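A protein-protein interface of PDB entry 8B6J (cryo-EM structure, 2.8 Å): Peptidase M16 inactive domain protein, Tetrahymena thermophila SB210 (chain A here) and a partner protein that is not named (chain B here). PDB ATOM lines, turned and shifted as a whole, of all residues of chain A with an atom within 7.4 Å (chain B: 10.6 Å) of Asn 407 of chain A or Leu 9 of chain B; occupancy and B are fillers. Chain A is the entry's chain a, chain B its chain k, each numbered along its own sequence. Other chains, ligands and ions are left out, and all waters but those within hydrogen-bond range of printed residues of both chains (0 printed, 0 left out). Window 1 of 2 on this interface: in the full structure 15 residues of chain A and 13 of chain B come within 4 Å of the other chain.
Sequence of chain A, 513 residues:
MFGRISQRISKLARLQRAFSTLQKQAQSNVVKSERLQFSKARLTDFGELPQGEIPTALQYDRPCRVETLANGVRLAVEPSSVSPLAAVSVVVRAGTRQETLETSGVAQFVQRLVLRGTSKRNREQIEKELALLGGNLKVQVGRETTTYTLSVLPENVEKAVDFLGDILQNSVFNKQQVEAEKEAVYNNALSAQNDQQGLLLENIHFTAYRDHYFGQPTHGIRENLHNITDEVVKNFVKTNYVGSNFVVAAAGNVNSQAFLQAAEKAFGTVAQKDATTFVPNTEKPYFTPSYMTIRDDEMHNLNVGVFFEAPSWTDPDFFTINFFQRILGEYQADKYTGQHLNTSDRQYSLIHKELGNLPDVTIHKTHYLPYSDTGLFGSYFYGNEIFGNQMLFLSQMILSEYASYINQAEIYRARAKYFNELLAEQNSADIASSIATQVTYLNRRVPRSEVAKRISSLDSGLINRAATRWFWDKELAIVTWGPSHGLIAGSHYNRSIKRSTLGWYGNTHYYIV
O of Pro 4 of chain B lies within hydrogen-bond range of OH of Tyr 348 of chain A (3.0 Å). The side-chain amide nitrogen (ND2) of Asn 407 of chain A sits at hydrogen-bond distance from the side-chain carboxylate (OE1) of Glu 12 of chain B (2.7 Å).
The side-chain amino group of Lys 8 of chain B sits at hydrogen-bond distance from the side-chain hydroxyl of Tyr 2 of chain B. The side-chain hydroxyl (OH) of Tyr 405 of chain A lies within hydrogen-bond range of the side-chain amide nitrogen (ND2) of Asn 407 of chain A (3.1 Å). OE1 of Gln 347 of chain A lies close to O of Ser 349 of chain A, at 3.4 Å. The backbone NH (N) of Ala 409 of chain A lies within hydrogen-bond range of the side-chain amide oxygen (OD1) of Asn 407 of chain A (2.7 Å). O of Tyr 348 of chain A sits at hydrogen-bond distance from NH1 of Arg 413 of chain A (3.4 Å). The backbone carbonyl oxygen (O) of Leu 9 of chain B lies within hydrogen-bond range of the side-chain hydroxyl (OG1) of Thr 13 of chain B (3.0 Å).
Among the printed residues, merely in contact across the chains: Tyr 412 of chain A with Tyr 2 of chain B, Tyr 405 of chain A with Glu 12 of chain B, Gln 347 of chain A with Phe 6 of chain B, Tyr 405 of chain A with Phe 16 of chain B, Tyr 348 of chain A with Leu 3 of chain B, Tyr 348 of chain A with Phe 6 of chain B, Ala 409 of chain A with Pro 4 of chain B, Tyr 348 of chain A with Leu 9 of chain B, Asn 407 of chain A with Leu 9 of chain B and Tyr 405 of chain A with Thr 13 of chain B.
Of chain B, only Leu 3 (3.5 Å), Pro 4 (3.0 Å), Phe 6 (3.6 Å) and Leu 9 (3.8 Å) come within 4 Å of Tyr 348 of chain A. Ile 406 of chain A touches none of the printed residues of chain B. Of chain B, only Leu 9 (3.8 Å) and Glu 12 (2.7 Å) come within 4 Å of Asn 407 of chain A. No residue of chain B comes within 4 Å of Gln 408 of chain A. Of the printed residues of chain A, Tyr 2 of chain B touches Tyr 412 (3.3 Å). Printed residues of chain A within 4 Å of Phe 6 of chain B: Gln 347 (3.5 Å) and Tyr 348 (3.6 Å). Of chain A, only Tyr 348 and Asn 407 come within 4 Å of Leu 9 of chain B. Of the printed residues of chain A, Thr 13 of chain B touches Tyr 405. Of the printed residues of chain A, Phe 16 of chain B touches Tyr 405 (3.5 Å). The nearest residue of chain A that does not touch Leu 9 of chain B is Gln 347 of chain A (4.4 Å).
Hydrophobic or aromatic side chains of chain B that line the printed part of chain A: Tyr 2, Leu 3, Pro 4, Phe 6, Leu 9 and Phe 16. Of the 17 printed residues of chain A, 6 touch a printed residue of chain B. Hydrophobic or aromatic side chains of chain A within 4 Å of the printed part of chain B: Tyr 348, Tyr 405, Ala 409 and Tyr 412. Among the printed residues, 12 pairs touch across the chains.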
ATOM      1  N   ILE A 327      -7.212 -11.627   4.246  1.00  0.00           N
ATOM      2  CA  ILE A 327      -8.478 -12.102   4.800  1.00  0.00           C
ATOM      3  C   ILE A 327      -9.559 -12.093   3.729  1.00  0.00           C
ATOM      4  O   ILE A 327     -10.263 -13.088   3.524  1.00  0.00           O
ATOM      5  CB  ILE A 327      -8.890 -11.250   6.015  1.00  0.00           C
ATOM      6  CG1 ILE A 327      -8.062 -11.632   7.242  1.00  0.00           C
ATOM      7  CG2 ILE A 327     -10.384 -11.412   6.294  1.00  0.00           C
ATOM      8  CD1 ILE A 327      -8.305 -10.745   8.446  1.00  0.00           C
ATOM      9  N   ASP A 345     -22.063 -22.366   2.979  1.00  0.00           N
ATOM     10  CA  ASP A 345     -21.868 -22.182   4.411  1.00  0.00           C
ATOM     11  C   ASP A 345     -20.689 -22.982   4.945  1.00  0.00           C
ATOM     12  O   ASP A 345     -20.119 -22.606   5.974  1.00  0.00           O
ATOM     13  CB  ASP A 345     -23.136 -22.581   5.166  1.00  0.00           C
ATOM     14  CG  ASP A 345     -24.386 -21.959   4.579  1.00  0.00           C
ATOM     15  OD1 ASP A 345     -24.270 -21.208   3.589  1.00  0.00           O
ATOM     16  OD2 ASP A 345     -25.487 -22.228   5.104  1.00  0.00           O
ATOM     17  N   GLN A 347     -17.398 -23.471   4.976  1.00  0.00           N
ATOM     18  CA  GLN A 347     -16.064 -22.944   4.718  1.00  0.00           C
ATOM     19  C   GLN A 347     -15.729 -21.980   5.847  1.00  0.00           C
ATOM     20  O   GLN A 347     -16.497 -21.821   6.800  1.00  0.00           O
ATOM     21  CB  GLN A 347     -15.978 -22.256   3.356  1.00  0.00           C
ATOM     22  CG  GLN A 347     -16.732 -20.939   3.281  1.00  0.00           C
ATOM     23  CD  GLN A 347     -16.648 -20.293   1.917  1.00  0.00           C
ATOM     24  OE1 GLN A 347     -17.615 -19.700   1.443  1.00  0.00           O
ATOM     25  NE2 GLN A 347     -15.486 -20.393   1.280  1.00  0.00           N
ATOM     26  N   TYR A 348     -14.572 -21.330   5.729  1.00  0.00           N
ATOM     27  CA  TYR A 348     -14.111 -20.384   6.733  1.00  0.00           C
ATOM     28  C   TYR A 348     -13.880 -18.987   6.179  1.00  0.00           C
ATOM     29  O   TYR A 348     -13.411 -18.116   6.920  1.00  0.00           O
ATOM     30  CB  TYR A 348     -12.825 -20.902   7.387  1.00  0.00           C
ATOM     31  CG  TYR A 348     -12.967 -22.299   7.940  1.00  0.00           C
ATOM     32  CD1 TYR A 348     -13.695 -22.534   9.097  1.00  0.00           C
ATOM     33  CD2 TYR A 348     -12.380 -23.382   7.305  1.00  0.00           C
ATOM     34  CE1 TYR A 348     -13.832 -23.808   9.606  1.00  0.00           C
ATOM     35  CE2 TYR A 348     -12.510 -24.659   7.807  1.00  0.00           C
ATOM     36  CZ  TYR A 348     -13.237 -24.866   8.958  1.00  0.00           C
ATOM     37  OH  TYR A 348     -13.370 -26.138   9.462  1.00  0.00           O
ATOM     38  N   SER A 349     -14.193 -18.746   4.909  1.00  0.00           N
ATOM     39  CA  SER A 349     -14.126 -17.416   4.318  1.00  0.00           C
ATOM     40  C   SER A 349     -15.536 -16.848   4.251  1.00  0.00           C
ATOM     41  O   SER A 349     -16.402 -17.404   3.566  1.00  0.00           O
ATOM     42  CB  SER A 349     -13.496 -17.465   2.927  1.00  0.00           C
ATOM     43  OG  SER A 349     -13.515 -16.187   2.316  1.00  0.00           O
ATOM     44  N   TYR A 402     -15.811  -6.905  10.565  1.00  0.00           N
ATOM     45  CA  TYR A 402     -14.594  -7.263  11.280  1.00  0.00           C
ATOM     46  C   TYR A 402     -14.263  -6.263  12.377  1.00  0.00           C
ATOM     47  O   TYR A 402     -13.484  -6.587  13.277  1.00  0.00           O
ATOM     48  CB  TYR A 402     -13.423  -7.376  10.302  1.00  0.00           C
ATOM     49  CG  TYR A 402     -13.587  -8.464   9.262  1.00  0.00           C
ATOM     50  CD1 TYR A 402     -14.446  -9.534   9.471  1.00  0.00           C
ATOM     51  CD2 TYR A 402     -12.877  -8.421   8.070  1.00  0.00           C
ATOM     52  CE1 TYR A 402     -14.595 -10.526   8.528  1.00  0.00           C
ATOM     53  CE2 TYR A 402     -13.021  -9.410   7.119  1.00  0.00           C
ATOM     54  CZ  TYR A 402     -13.881 -10.461   7.353  1.00  0.00           C
ATOM     55  OH  TYR A 402     -14.030 -11.452   6.410  1.00  0.00           O
ATOM     56  N   TYR A 405     -16.538  -8.124  15.215  1.00  0.00           N
ATOM     57  CA  TYR A 405     -16.270  -9.521  15.531  1.00  0.00           C
ATOM     58  C   TYR A 405     -15.669 -10.207  14.316  1.00  0.00           C
ATOM     59  O   TYR A 405     -16.222 -10.119  13.217  1.00  0.00           O
ATOM     60  CB  TYR A 405     -17.551 -10.238  15.963  1.00  0.00           C
ATOM     61  CG  TYR A 405     -17.422 -11.743  16.027  1.00  0.00           C
ATOM     62  CD1 TYR A 405     -16.818 -12.363  17.112  1.00  0.00           C
ATOM     63  CD2 TYR A 405     -17.908 -12.546  15.004  1.00  0.00           C
ATOM     64  CE1 TYR A 405     -16.697 -13.735  17.175  1.00  0.00           C
ATOM     65  CE2 TYR A 405     -17.792 -13.920  15.058  1.00  0.00           C
ATOM     66  CZ  TYR A 405     -17.186 -14.508  16.147  1.00  0.00           C
ATOM     67  OH  TYR A 405     -17.067 -15.877  16.208  1.00  0.00           O
ATOM     68  N   ILE A 406     -14.544 -10.887  14.520  1.00  0.00           N
ATOM     69  CA  ILE A 406     -13.925 -11.718  13.496  1.00  0.00           C
ATOM     70  C   ILE A 406     -13.606 -13.069  14.119  1.00  0.00           C
ATOM     71  O   ILE A 406     -13.027 -13.134  15.209  1.00  0.00           O
ATOM     72  CB  ILE A 406     -12.654 -11.070  12.914  1.00  0.00           C
ATOM     73  CG1 ILE A 406     -12.137 -11.894  11.732  1.00  0.00           C
ATOM     74  CG2 ILE A 406     -11.582 -10.942  13.981  1.00  0.00           C
ATOM     75  CD1 ILE A 406     -10.974 -11.263  11.011  1.00  0.00           C
ATOM     76  N   ASN A 407     -13.993 -14.142  13.436  1.00  0.00           N
ATOM     77  CA  ASN A 407     -13.763 -15.482  13.951  1.00  0.00           C
ATOM     78  C   ASN A 407     -12.287 -15.852  13.851  1.00  0.00           C
ATOM     79  O   ASN A 407     -11.578 -15.431  12.933  1.00  0.00           O
ATOM     80  CB  ASN A 407     -14.612 -16.496  13.183  1.00  0.00           C
ATOM     81  CG  ASN A 407     -14.582 -17.874  13.809  1.00  0.00           C
ATOM     82  OD1 ASN A 407     -13.730 -18.698  13.484  1.00  0.00           O
ATOM     83  ND2 ASN A 407     -15.518 -18.130  14.714  1.00  0.00           N
ATOM     84  N   GLN A 408     -11.824 -16.652  14.814  1.00  0.00           N
ATOM     85  CA  GLN A 408     -10.429 -17.080  14.806  1.00  0.00           C
ATOM     86  C   GLN A 408     -10.110 -17.921  13.577  1.00  0.00           C
ATOM     87  O   GLN A 408      -8.956 -17.959  13.132  1.00  0.00           O
ATOM     88  CB  GLN A 408     -10.107 -17.861  16.080  1.00  0.00           C
ATOM     89  CG  GLN A 408      -9.058 -17.200  16.960  1.00  0.00           C
ATOM     90  CD  GLN A 408      -7.697 -17.144  16.303  1.00  0.00           C
ATOM     91  OE1 GLN A 408      -7.483 -17.731  15.245  1.00  0.00           O
ATOM     92  NE2 GLN A 408      -6.766 -16.437  16.930  1.00  0.00           N
ATOM     93  N   ALA A 409     -11.112 -18.599  13.015  1.00  0.00           N
ATOM     94  CA  ALA A 409     -10.874 -19.393  11.816  1.00  0.00           C
ATOM     95  C   ALA A 409     -10.387 -18.517  10.670  1.00  0.00           C
ATOM     96  O   ALA A 409      -9.444 -18.879   9.959  1.00  0.00           O
ATOM     97  CB  ALA A 409     -12.147 -20.138  11.419  1.00  0.00           C
ATOM     98  N   GLU A 410     -11.013 -17.355  10.479  1.00  0.00           N
ATOM     99  CA  GLU A 410     -10.560 -16.436   9.441  1.00  0.00           C
ATOM    100  C   GLU A 410      -9.164 -15.908   9.741  1.00  0.00           C
ATOM    101  O   GLU A 410      -8.339 -15.761   8.831  1.00  0.00           O
ATOM    102  CB  GLU A 410     -11.548 -15.282   9.296  1.00  0.00           C
ATOM    103  CG  GLU A 410     -12.844 -15.664   8.609  1.00  0.00           C
ATOM    104  CD  GLU A 410     -13.836 -14.522   8.566  1.00  0.00           C
ATOM    105  OE1 GLU A 410     -14.041 -13.873   9.613  1.00  0.00           O
ATOM    106  OE2 GLU A 410     -14.403 -14.267   7.484  1.00  0.00           O
ATOM    107  N   ILE A 411      -8.883 -15.611  11.012  1.00  0.00           N
ATOM    108  CA  ILE A 411      -7.560 -15.116  11.380  1.00  0.00           C
ATOM    109  C   ILE A 411      -6.496 -16.128  10.983  1.00  0.00           C
ATOM    110  O   ILE A 411      -5.492 -15.786  10.349  1.00  0.00           O
ATOM    111  CB  ILE A 411      -7.500 -14.804  12.886  1.00  0.00           C
ATOM    112  CG1 ILE A 411      -8.516 -13.719  13.249  1.00  0.00           C
ATOM    113  CG2 ILE A 411      -6.092 -14.374  13.282  1.00  0.00           C
ATOM    114  CD1 ILE A 411      -8.629 -13.463  14.734  1.00  0.00           C
ATOM    115  N   TYR A 412      -6.711 -17.398  11.336  1.00  0.00           N
ATOM    116  CA  TYR A 412      -5.718 -18.419  11.023  1.00  0.00           C
ATOM    117  C   TYR A 412      -5.662 -18.721   9.531  1.00  0.00           C
ATOM    118  O   TYR A 412      -4.582 -19.012   9.005  1.00  0.00           O
ATOM    119  CB  TYR A 412      -6.007 -19.691  11.819  1.00  0.00           C
ATOM    120  CG  TYR A 412      -5.615 -19.620  13.284  1.00  0.00           C
ATOM    121  CD1 TYR A 412      -4.540 -18.849  13.708  1.00  0.00           C
ATOM    122  CD2 TYR A 412      -6.316 -20.336  14.240  1.00  0.00           C
ATOM    123  CE1 TYR A 412      -4.182 -18.792  15.039  1.00  0.00           C
ATOM    124  CE2 TYR A 412      -5.965 -20.284  15.574  1.00  0.00           C
ATOM    125  CZ  TYR A 412      -4.898 -19.511  15.967  1.00  0.00           C
ATOM    126  OH  TYR A 412      -4.545 -19.456  17.295  1.00  0.00           O
ATOM    127  N   ARG A 413      -6.794 -18.653   8.829  1.00  0.00           N
ATOM    128  CA  ARG A 413      -6.767 -18.841   7.383  1.00  0.00           C
ATOM    129  C   ARG A 413      -5.900 -17.781   6.718  1.00  0.00           C
ATOM    130  O   ARG A 413      -5.042 -18.094   5.885  1.00  0.00           O
ATOM    131  CB  ARG A 413      -8.186 -18.796   6.816  1.00  0.00           C
ATOM    132  CG  ARG A 413      -8.267 -19.160   5.343  1.00  0.00           C
ATOM    133  CD  ARG A 413      -9.616 -18.810   4.742  1.00  0.00           C
ATOM    134  NE  ARG A 413      -9.649 -17.457   4.197  1.00  0.00           N
ATOM    135  CZ  ARG A 413     -10.107 -16.390   4.838  1.00  0.00           C
ATOM    136  NH1 ARG A 413     -10.578 -16.469   6.072  1.00  0.00           N
ATOM    137  NH2 ARG A 413     -10.096 -15.211   4.224  1.00  0.00           N
ATOM    138  N   SER A 460      -7.567 -11.239  17.323  1.00  0.00           N
ATOM    139  CA  SER A 460      -8.930 -10.821  17.015  1.00  0.00           C
ATOM    140  C   SER A 460      -9.199  -9.415  17.536  1.00  0.00           C
ATOM    141  O   SER A 460      -9.817  -8.597  16.844  1.00  0.00           O
ATOM    142  CB  SER A 460      -9.932 -11.814  17.603  1.00  0.00           C
ATOM    143  OG  SER A 460      -9.847 -11.848  19.016  1.00  0.00           O
ATOM    144  N   ASN A 464      -9.977  -6.193  15.248  1.00  0.00           N
ATOM    145  CA  ASN A 464     -11.154  -5.350  15.427  1.00  0.00           C
ATOM    146  C   ASN A 464     -10.763  -3.886  15.562  1.00  0.00           C
ATOM    147  O   ASN A 464     -11.401  -3.007  14.971  1.00  0.00           O
ATOM    148  CB  ASN A 464     -11.941  -5.799  16.658  1.00  0.00           C
ATOM    149  CG  ASN A 464     -12.432  -7.227  16.551  1.00  0.00           C
ATOM    150  OD1 ASN A 464     -12.241  -8.030  17.464  1.00  0.00           O
ATOM    151  ND2 ASN A 464     -13.073  -7.551  15.437  1.00  0.00           N
ATOM    152  N   TYR B   2      -6.102 -25.365  11.702  1.00  0.00           N
ATOM    153  CA  TYR B   2      -7.266 -25.031  12.513  1.00  0.00           C
ATOM    154  C   TYR B   2      -8.520 -25.336  11.700  1.00  0.00           C
ATOM    155  O   TYR B   2      -8.814 -24.645  10.719  1.00  0.00           O
ATOM    156  CB  TYR B   2      -7.214 -23.561  12.924  1.00  0.00           C
ATOM    157  CG  TYR B   2      -8.013 -23.217  14.159  1.00  0.00           C
ATOM    158  CD1 TYR B   2      -7.624 -23.671  15.410  1.00  0.00           C
ATOM    159  CD2 TYR B   2      -9.138 -22.410  14.080  1.00  0.00           C
ATOM    160  CE1 TYR B   2      -8.344 -23.349  16.542  1.00  0.00           C
ATOM    161  CE2 TYR B   2      -9.865 -22.084  15.205  1.00  0.00           C
ATOM    162  CZ  TYR B   2      -9.463 -22.555  16.433  1.00  0.00           C
ATOM    163  OH  TYR B   2     -10.186 -22.230  17.557  1.00  0.00           O
ATOM    164  N   LEU B   3      -9.261 -26.362  12.113  1.00  0.00           N
ATOM    165  CA  LEU B   3     -10.467 -26.808  11.415  1.00  0.00           C
ATOM    166  C   LEU B   3     -11.617 -26.858  12.411  1.00  0.00           C
ATOM    167  O   LEU B   3     -12.112 -27.937  12.760  1.00  0.00           O
ATOM    168  CB  LEU B   3     -10.258 -28.177  10.765  1.00  0.00           C
ATOM    169  CG  LEU B   3      -9.092 -28.315   9.787  1.00  0.00           C
ATOM    170  CD1 LEU B   3      -9.052 -29.719   9.212  1.00  0.00           C
ATOM    171  CD2 LEU B   3      -9.188 -27.288   8.677  1.00  0.00           C
ATOM    172  N   PRO B   4     -12.071 -25.703  12.887  1.00  0.00           N
ATOM    173  CA  PRO B   4     -13.164 -25.691  13.861  1.00  0.00           C
ATOM    174  C   PRO B   4     -14.457 -26.212  13.259  1.00  0.00           C
ATOM    175  O   PRO B   4     -14.739 -26.030  12.073  1.00  0.00           O
ATOM    176  CB  PRO B   4     -13.279 -24.212  14.245  1.00  0.00           C
ATOM    177  CG  PRO B   4     -12.743 -23.479  13.074  1.00  0.00           C
ATOM    178  CD  PRO B   4     -11.667 -24.345  12.490  1.00  0.00           C
ATOM    179  N   THR B   5     -15.249 -26.870  14.099  1.00  0.00           N
ATOM    180  CA  THR B   5     -16.532 -27.395  13.657  1.00  0.00           C
ATOM    181  C   THR B   5     -17.518 -26.256  13.440  1.00  0.00           C
ATOM    182  O   THR B   5     -17.572 -25.301  14.219  1.00  0.00           O
ATOM    183  CB  THR B   5     -17.083 -28.384  14.683  1.00  0.00           C
ATOM    184  OG1 THR B   5     -16.081 -29.357  14.997  1.00  0.00           O
ATOM    185  CG2 THR B   5     -18.305 -29.095  14.137  1.00  0.00           C
ATOM    186  N   PHE B   6     -18.306 -26.360  12.367  1.00  0.00           N
ATOM    187  CA  PHE B   6     -19.251 -25.297  12.045  1.00  0.00           C
ATOM    188  C   PHE B   6     -20.275 -25.104  13.155  1.00  0.00           C
ATOM    189  O   PHE B   6     -20.825 -24.007  13.309  1.00  0.00           O
ATOM    190  CB  PHE B   6     -19.940 -25.604  10.717  1.00  0.00           C
ATOM    191  CG  PHE B   6     -18.990 -25.711   9.557  1.00  0.00           C
ATOM    192  CD1 PHE B   6     -17.916 -24.846   9.442  1.00  0.00           C
ATOM    193  CD2 PHE B   6     -19.163 -26.685   8.590  1.00  0.00           C
ATOM    194  CE1 PHE B   6     -17.039 -24.943   8.382  1.00  0.00           C
ATOM    195  CE2 PHE B   6     -18.287 -26.789   7.527  1.00  0.00           C
ATOM    196  CZ  PHE B   6     -17.224 -25.916   7.424  1.00  0.00           C
ATOM    197  N   TYR B   7     -20.542 -26.149  13.941  1.00  0.00           N
ATOM    198  CA  TYR B   7     -21.305 -25.966  15.169  1.00  0.00           C
ATOM    199  C   TYR B   7     -20.680 -24.872  16.023  1.00  0.00           C
ATOM    200  O   TYR B   7     -21.368 -23.962  16.499  1.00  0.00           O
ATOM    201  CB  TYR B   7     -21.361 -27.273  15.961  1.00  0.00           C
ATOM    202  CG  TYR B   7     -22.345 -28.302  15.452  1.00  0.00           C
ATOM    203  CD1 TYR B   7     -23.703 -28.027  15.406  1.00  0.00           C
ATOM    204  CD2 TYR B   7     -21.918 -29.560  15.055  1.00  0.00           C
ATOM    205  CE1 TYR B   7     -24.605 -28.969  14.955  1.00  0.00           C
ATOM    206  CE2 TYR B   7     -22.815 -30.507  14.605  1.00  0.00           C
ATOM    207  CZ  TYR B   7     -24.156 -30.207  14.558  1.00  0.00           C
ATOM    208  OH  TYR B   7     -25.056 -31.145  14.113  1.00  0.00           O
ATOM    209  N   LYS B   8     -19.363 -24.953  16.228  1.00  0.00           N
ATOM    210  CA  LYS B   8     -18.682 -23.977  17.069  1.00  0.00           C
ATOM    211  C   LYS B   8     -18.733 -22.585  16.455  1.00  0.00           C
ATOM    212  O   LYS B   8     -18.914 -21.595  17.172  1.00  0.00           O
ATOM    213  CB  LYS B   8     -17.235 -24.405  17.304  1.00  0.00           C
ATOM    214  CG  LYS B   8     -16.478 -23.474  18.230  1.00  0.00           C
ATOM    215  CD  LYS B   8     -15.100 -23.998  18.563  1.00  0.00           C
ATOM    216  CE  LYS B   8     -14.193 -23.959  17.357  1.00  0.00           C
ATOM    217  NZ  LYS B   8     -12.783 -24.200  17.742  1.00  0.00           N
ATOM    218  N   LEU B   9     -18.554 -22.483  15.137  1.00  0.00           N
ATOM    219  CA  LEU B   9     -18.624 -21.175  14.495  1.00  0.00           C
ATOM    220  C   LEU B   9     -19.999 -20.550  14.676  1.00  0.00           C
ATOM    221  O   LEU B   9     -20.113 -19.360  14.997  1.00  0.00           O
ATOM    222  CB  LEU B   9     -18.284 -21.297  13.010  1.00  0.00           C
ATOM    223  CG  LEU B   9     -16.811 -21.092  12.661  1.00  0.00           C
ATOM    224  CD1 LEU B   9     -15.935 -22.073  13.414  1.00  0.00           C
ATOM    225  CD2 LEU B   9     -16.597 -21.222  11.164  1.00  0.00           C
ATOM    226  N   PHE B  10     -21.059 -21.336  14.476  1.00  0.00           N
ATOM    227  CA  PHE B  10     -22.405 -20.812  14.673  1.00  0.00           C
ATOM    228  C   PHE B  10     -22.620 -20.390  16.119  1.00  0.00           C
ATOM    229  O   PHE B  10     -23.191 -19.325  16.386  1.00  0.00           O
ATOM    230  CB  PHE B  10     -23.436 -21.859  14.259  1.00  0.00           C
ATOM    231  CG  PHE B  10     -24.852 -21.372  14.321  1.00  0.00           C
ATOM    232  CD1 PHE B  10     -25.374 -20.592  13.306  1.00  0.00           C
ATOM    233  CD2 PHE B  10     -25.664 -21.699  15.391  1.00  0.00           C
ATOM    234  CE1 PHE B  10     -26.676 -20.144  13.361  1.00  0.00           C
ATOM    235  CE2 PHE B  10     -26.968 -21.252  15.448  1.00  0.00           C
ATOM    236  CZ  PHE B  10     -27.472 -20.475  14.434  1.00  0.00           C
ATOM    237  N   HIS B  11     -22.162 -21.209  17.068  1.00  0.00           N
ATOM    238  CA  HIS B  11     -22.332 -20.866  18.475  1.00  0.00           C
ATOM    239  C   HIS B  11     -21.618 -19.565  18.814  1.00  0.00           C
ATOM    240  O   HIS B  11     -22.176 -18.705  19.503  1.00  0.00           O
ATOM    241  CB  HIS B  11     -21.816 -22.002  19.357  1.00  0.00           C
ATOM    242  CG  HIS B  11     -22.603 -23.269  19.231  1.00  0.00           C
ATOM    243  ND1 HIS B  11     -23.755 -23.358  18.479  1.00  0.00           N
ATOM    244  CD2 HIS B  11     -22.405 -24.498  19.761  1.00  0.00           C
ATOM    245  CE1 HIS B  11     -24.232 -24.587  18.552  1.00  0.00           C
ATOM    246  NE2 HIS B  11     -23.431 -25.299  19.324  1.00  0.00           N
ATOM    247  N   GLU B  12     -20.385 -19.399  18.332  1.00  0.00           N
ATOM    248  CA  GLU B  12     -19.626 -18.191  18.637  1.00  0.00           C
ATOM    249  C   GLU B  12     -20.255 -16.961  17.992  1.00  0.00           C
ATOM    250  O   GLU B  12     -20.344 -15.898  18.620  1.00  0.00           O
ATOM    251  CB  GLU B  12     -18.181 -18.361  18.179  1.00  0.00           C
ATOM    252  CG  GLU B  12     -17.433 -19.455  18.917  1.00  0.00           C
ATOM    253  CD  GLU B  12     -16.092 -19.769  18.293  1.00  0.00           C
ATOM    254  OE1 GLU B  12     -15.790 -19.207  17.219  1.00  0.00           O
ATOM    255  OE2 GLU B  12     -15.339 -20.578  18.873  1.00  0.00           O
ATOM    256  N   THR B  13     -20.692 -17.081  16.735  1.00  0.00           N
ATOM    257  CA  THR B  13     -21.328 -15.948  16.075  1.00  0.00           C
ATOM    258  C   THR B  13     -22.608 -15.544  16.795  1.00  0.00           C
ATOM    259  O   THR B  13     -22.870 -14.351  16.990  1.00  0.00           O
ATOM    260  CB  THR B  13     -21.617 -16.287  14.613  1.00  0.00           C
ATOM    261  OG1 THR B  13     -20.391 -16.598  13.941  1.00  0.00           O
ATOM    262  CG2 THR B  13     -22.291 -15.118  13.914  1.00  0.00           C
ATOM    263  N   ASN B  14     -23.417 -16.524  17.203  1.00  0.00           N
ATOM    264  CA  ASN B  14     -24.636 -16.197  17.931  1.00  0.00           C
ATOM    265  C   ASN B  14     -24.330 -15.618  19.305  1.00  0.00           C
ATOM    266  O   ASN B  14     -25.060 -14.743  19.778  1.00  0.00           O
ATOM    267  CB  ASN B  14     -25.525 -17.430  18.055  1.00  0.00           C
ATOM    268  CG  ASN B  14     -26.204 -17.782  16.752  1.00  0.00           C
ATOM    269  OD1 ASN B  14     -25.635 -17.606  15.677  1.00  0.00           O
ATOM    270  ND2 ASN B  14     -27.435 -18.266  16.838  1.00  0.00           N
ATOM    271  N   ALA B  15     -23.265 -16.081  19.960  1.00  0.00           N
ATOM    272  CA  ALA B  15     -22.875 -15.479  21.230  1.00  0.00           C
ATOM    273  C   ALA B  15     -22.506 -14.014  21.045  1.00  0.00           C
ATOM    274  O   ALA B  15     -22.915 -13.156  21.836  1.00  0.00           O
ATOM    275  CB  ALA B  15     -21.708 -16.252  21.842  1.00  0.00           C
ATOM    276  N   PHE B  16     -21.738 -13.706  19.998  1.00  0.00           N
ATOM    277  CA  PHE B  16     -21.389 -12.312  19.738  1.00  0.00           C
ATOM    278  C   PHE B  16     -22.625 -11.479  19.420  1.00  0.00           C
ATOM    279  O   PHE B  16     -22.742 -10.335  19.871  1.00  0.00           O
ATOM    280  CB  PHE B  16     -20.389 -12.209  18.592  1.00  0.00           C
ATOM    281  CG  PHE B  16     -20.395 -10.869  17.923  1.00  0.00           C
ATOM    282  CD1 PHE B  16     -19.893  -9.756  18.572  1.00  0.00           C
ATOM    283  CD2 PHE B  16     -20.924 -10.716  16.654  1.00  0.00           C
ATOM    284  CE1 PHE B  16     -19.907  -8.519  17.963  1.00  0.00           C
ATOM    285  CE2 PHE B  16     -20.939  -9.483  16.041  1.00  0.00           C
ATOM    286  CZ  PHE B  16     -20.429  -8.383  16.697  1.00  0.00           C
ATOM    287  N   ARG B  17     -23.545 -12.021  18.621  1.00  0.00           N
ATOM    288  CA  ARG B  17     -24.750 -11.268  18.287  1.00  0.00           C
ATOM    289  C   ARG B  17     -25.612 -11.032  19.522  1.00  0.00           C
ATOM    290  O   ARG B  17     -26.211  -9.962  19.675  1.00  0.00           O
ATOM    291  CB  ARG B  17     -25.541 -11.996  17.202  1.00  0.00           C
ATOM    292  CG  ARG B  17     -24.860 -11.977  15.846  1.00  0.00           C
ATOM    293  CD  ARG B  17     -25.640 -12.766  14.813  1.00  0.00           C
ATOM    294  NE  ARG B  17     -24.969 -12.776  13.517  1.00  0.00           N
ATOM    295  CZ  ARG B  17     -25.145 -11.866  12.569  1.00  0.00           C
ATOM    296  NH1 ARG B  17     -25.981 -10.852  12.727  1.00  0.00           N
ATOM    297  NH2 ARG B  17     -24.465 -11.976  11.432  1.00  0.00           N
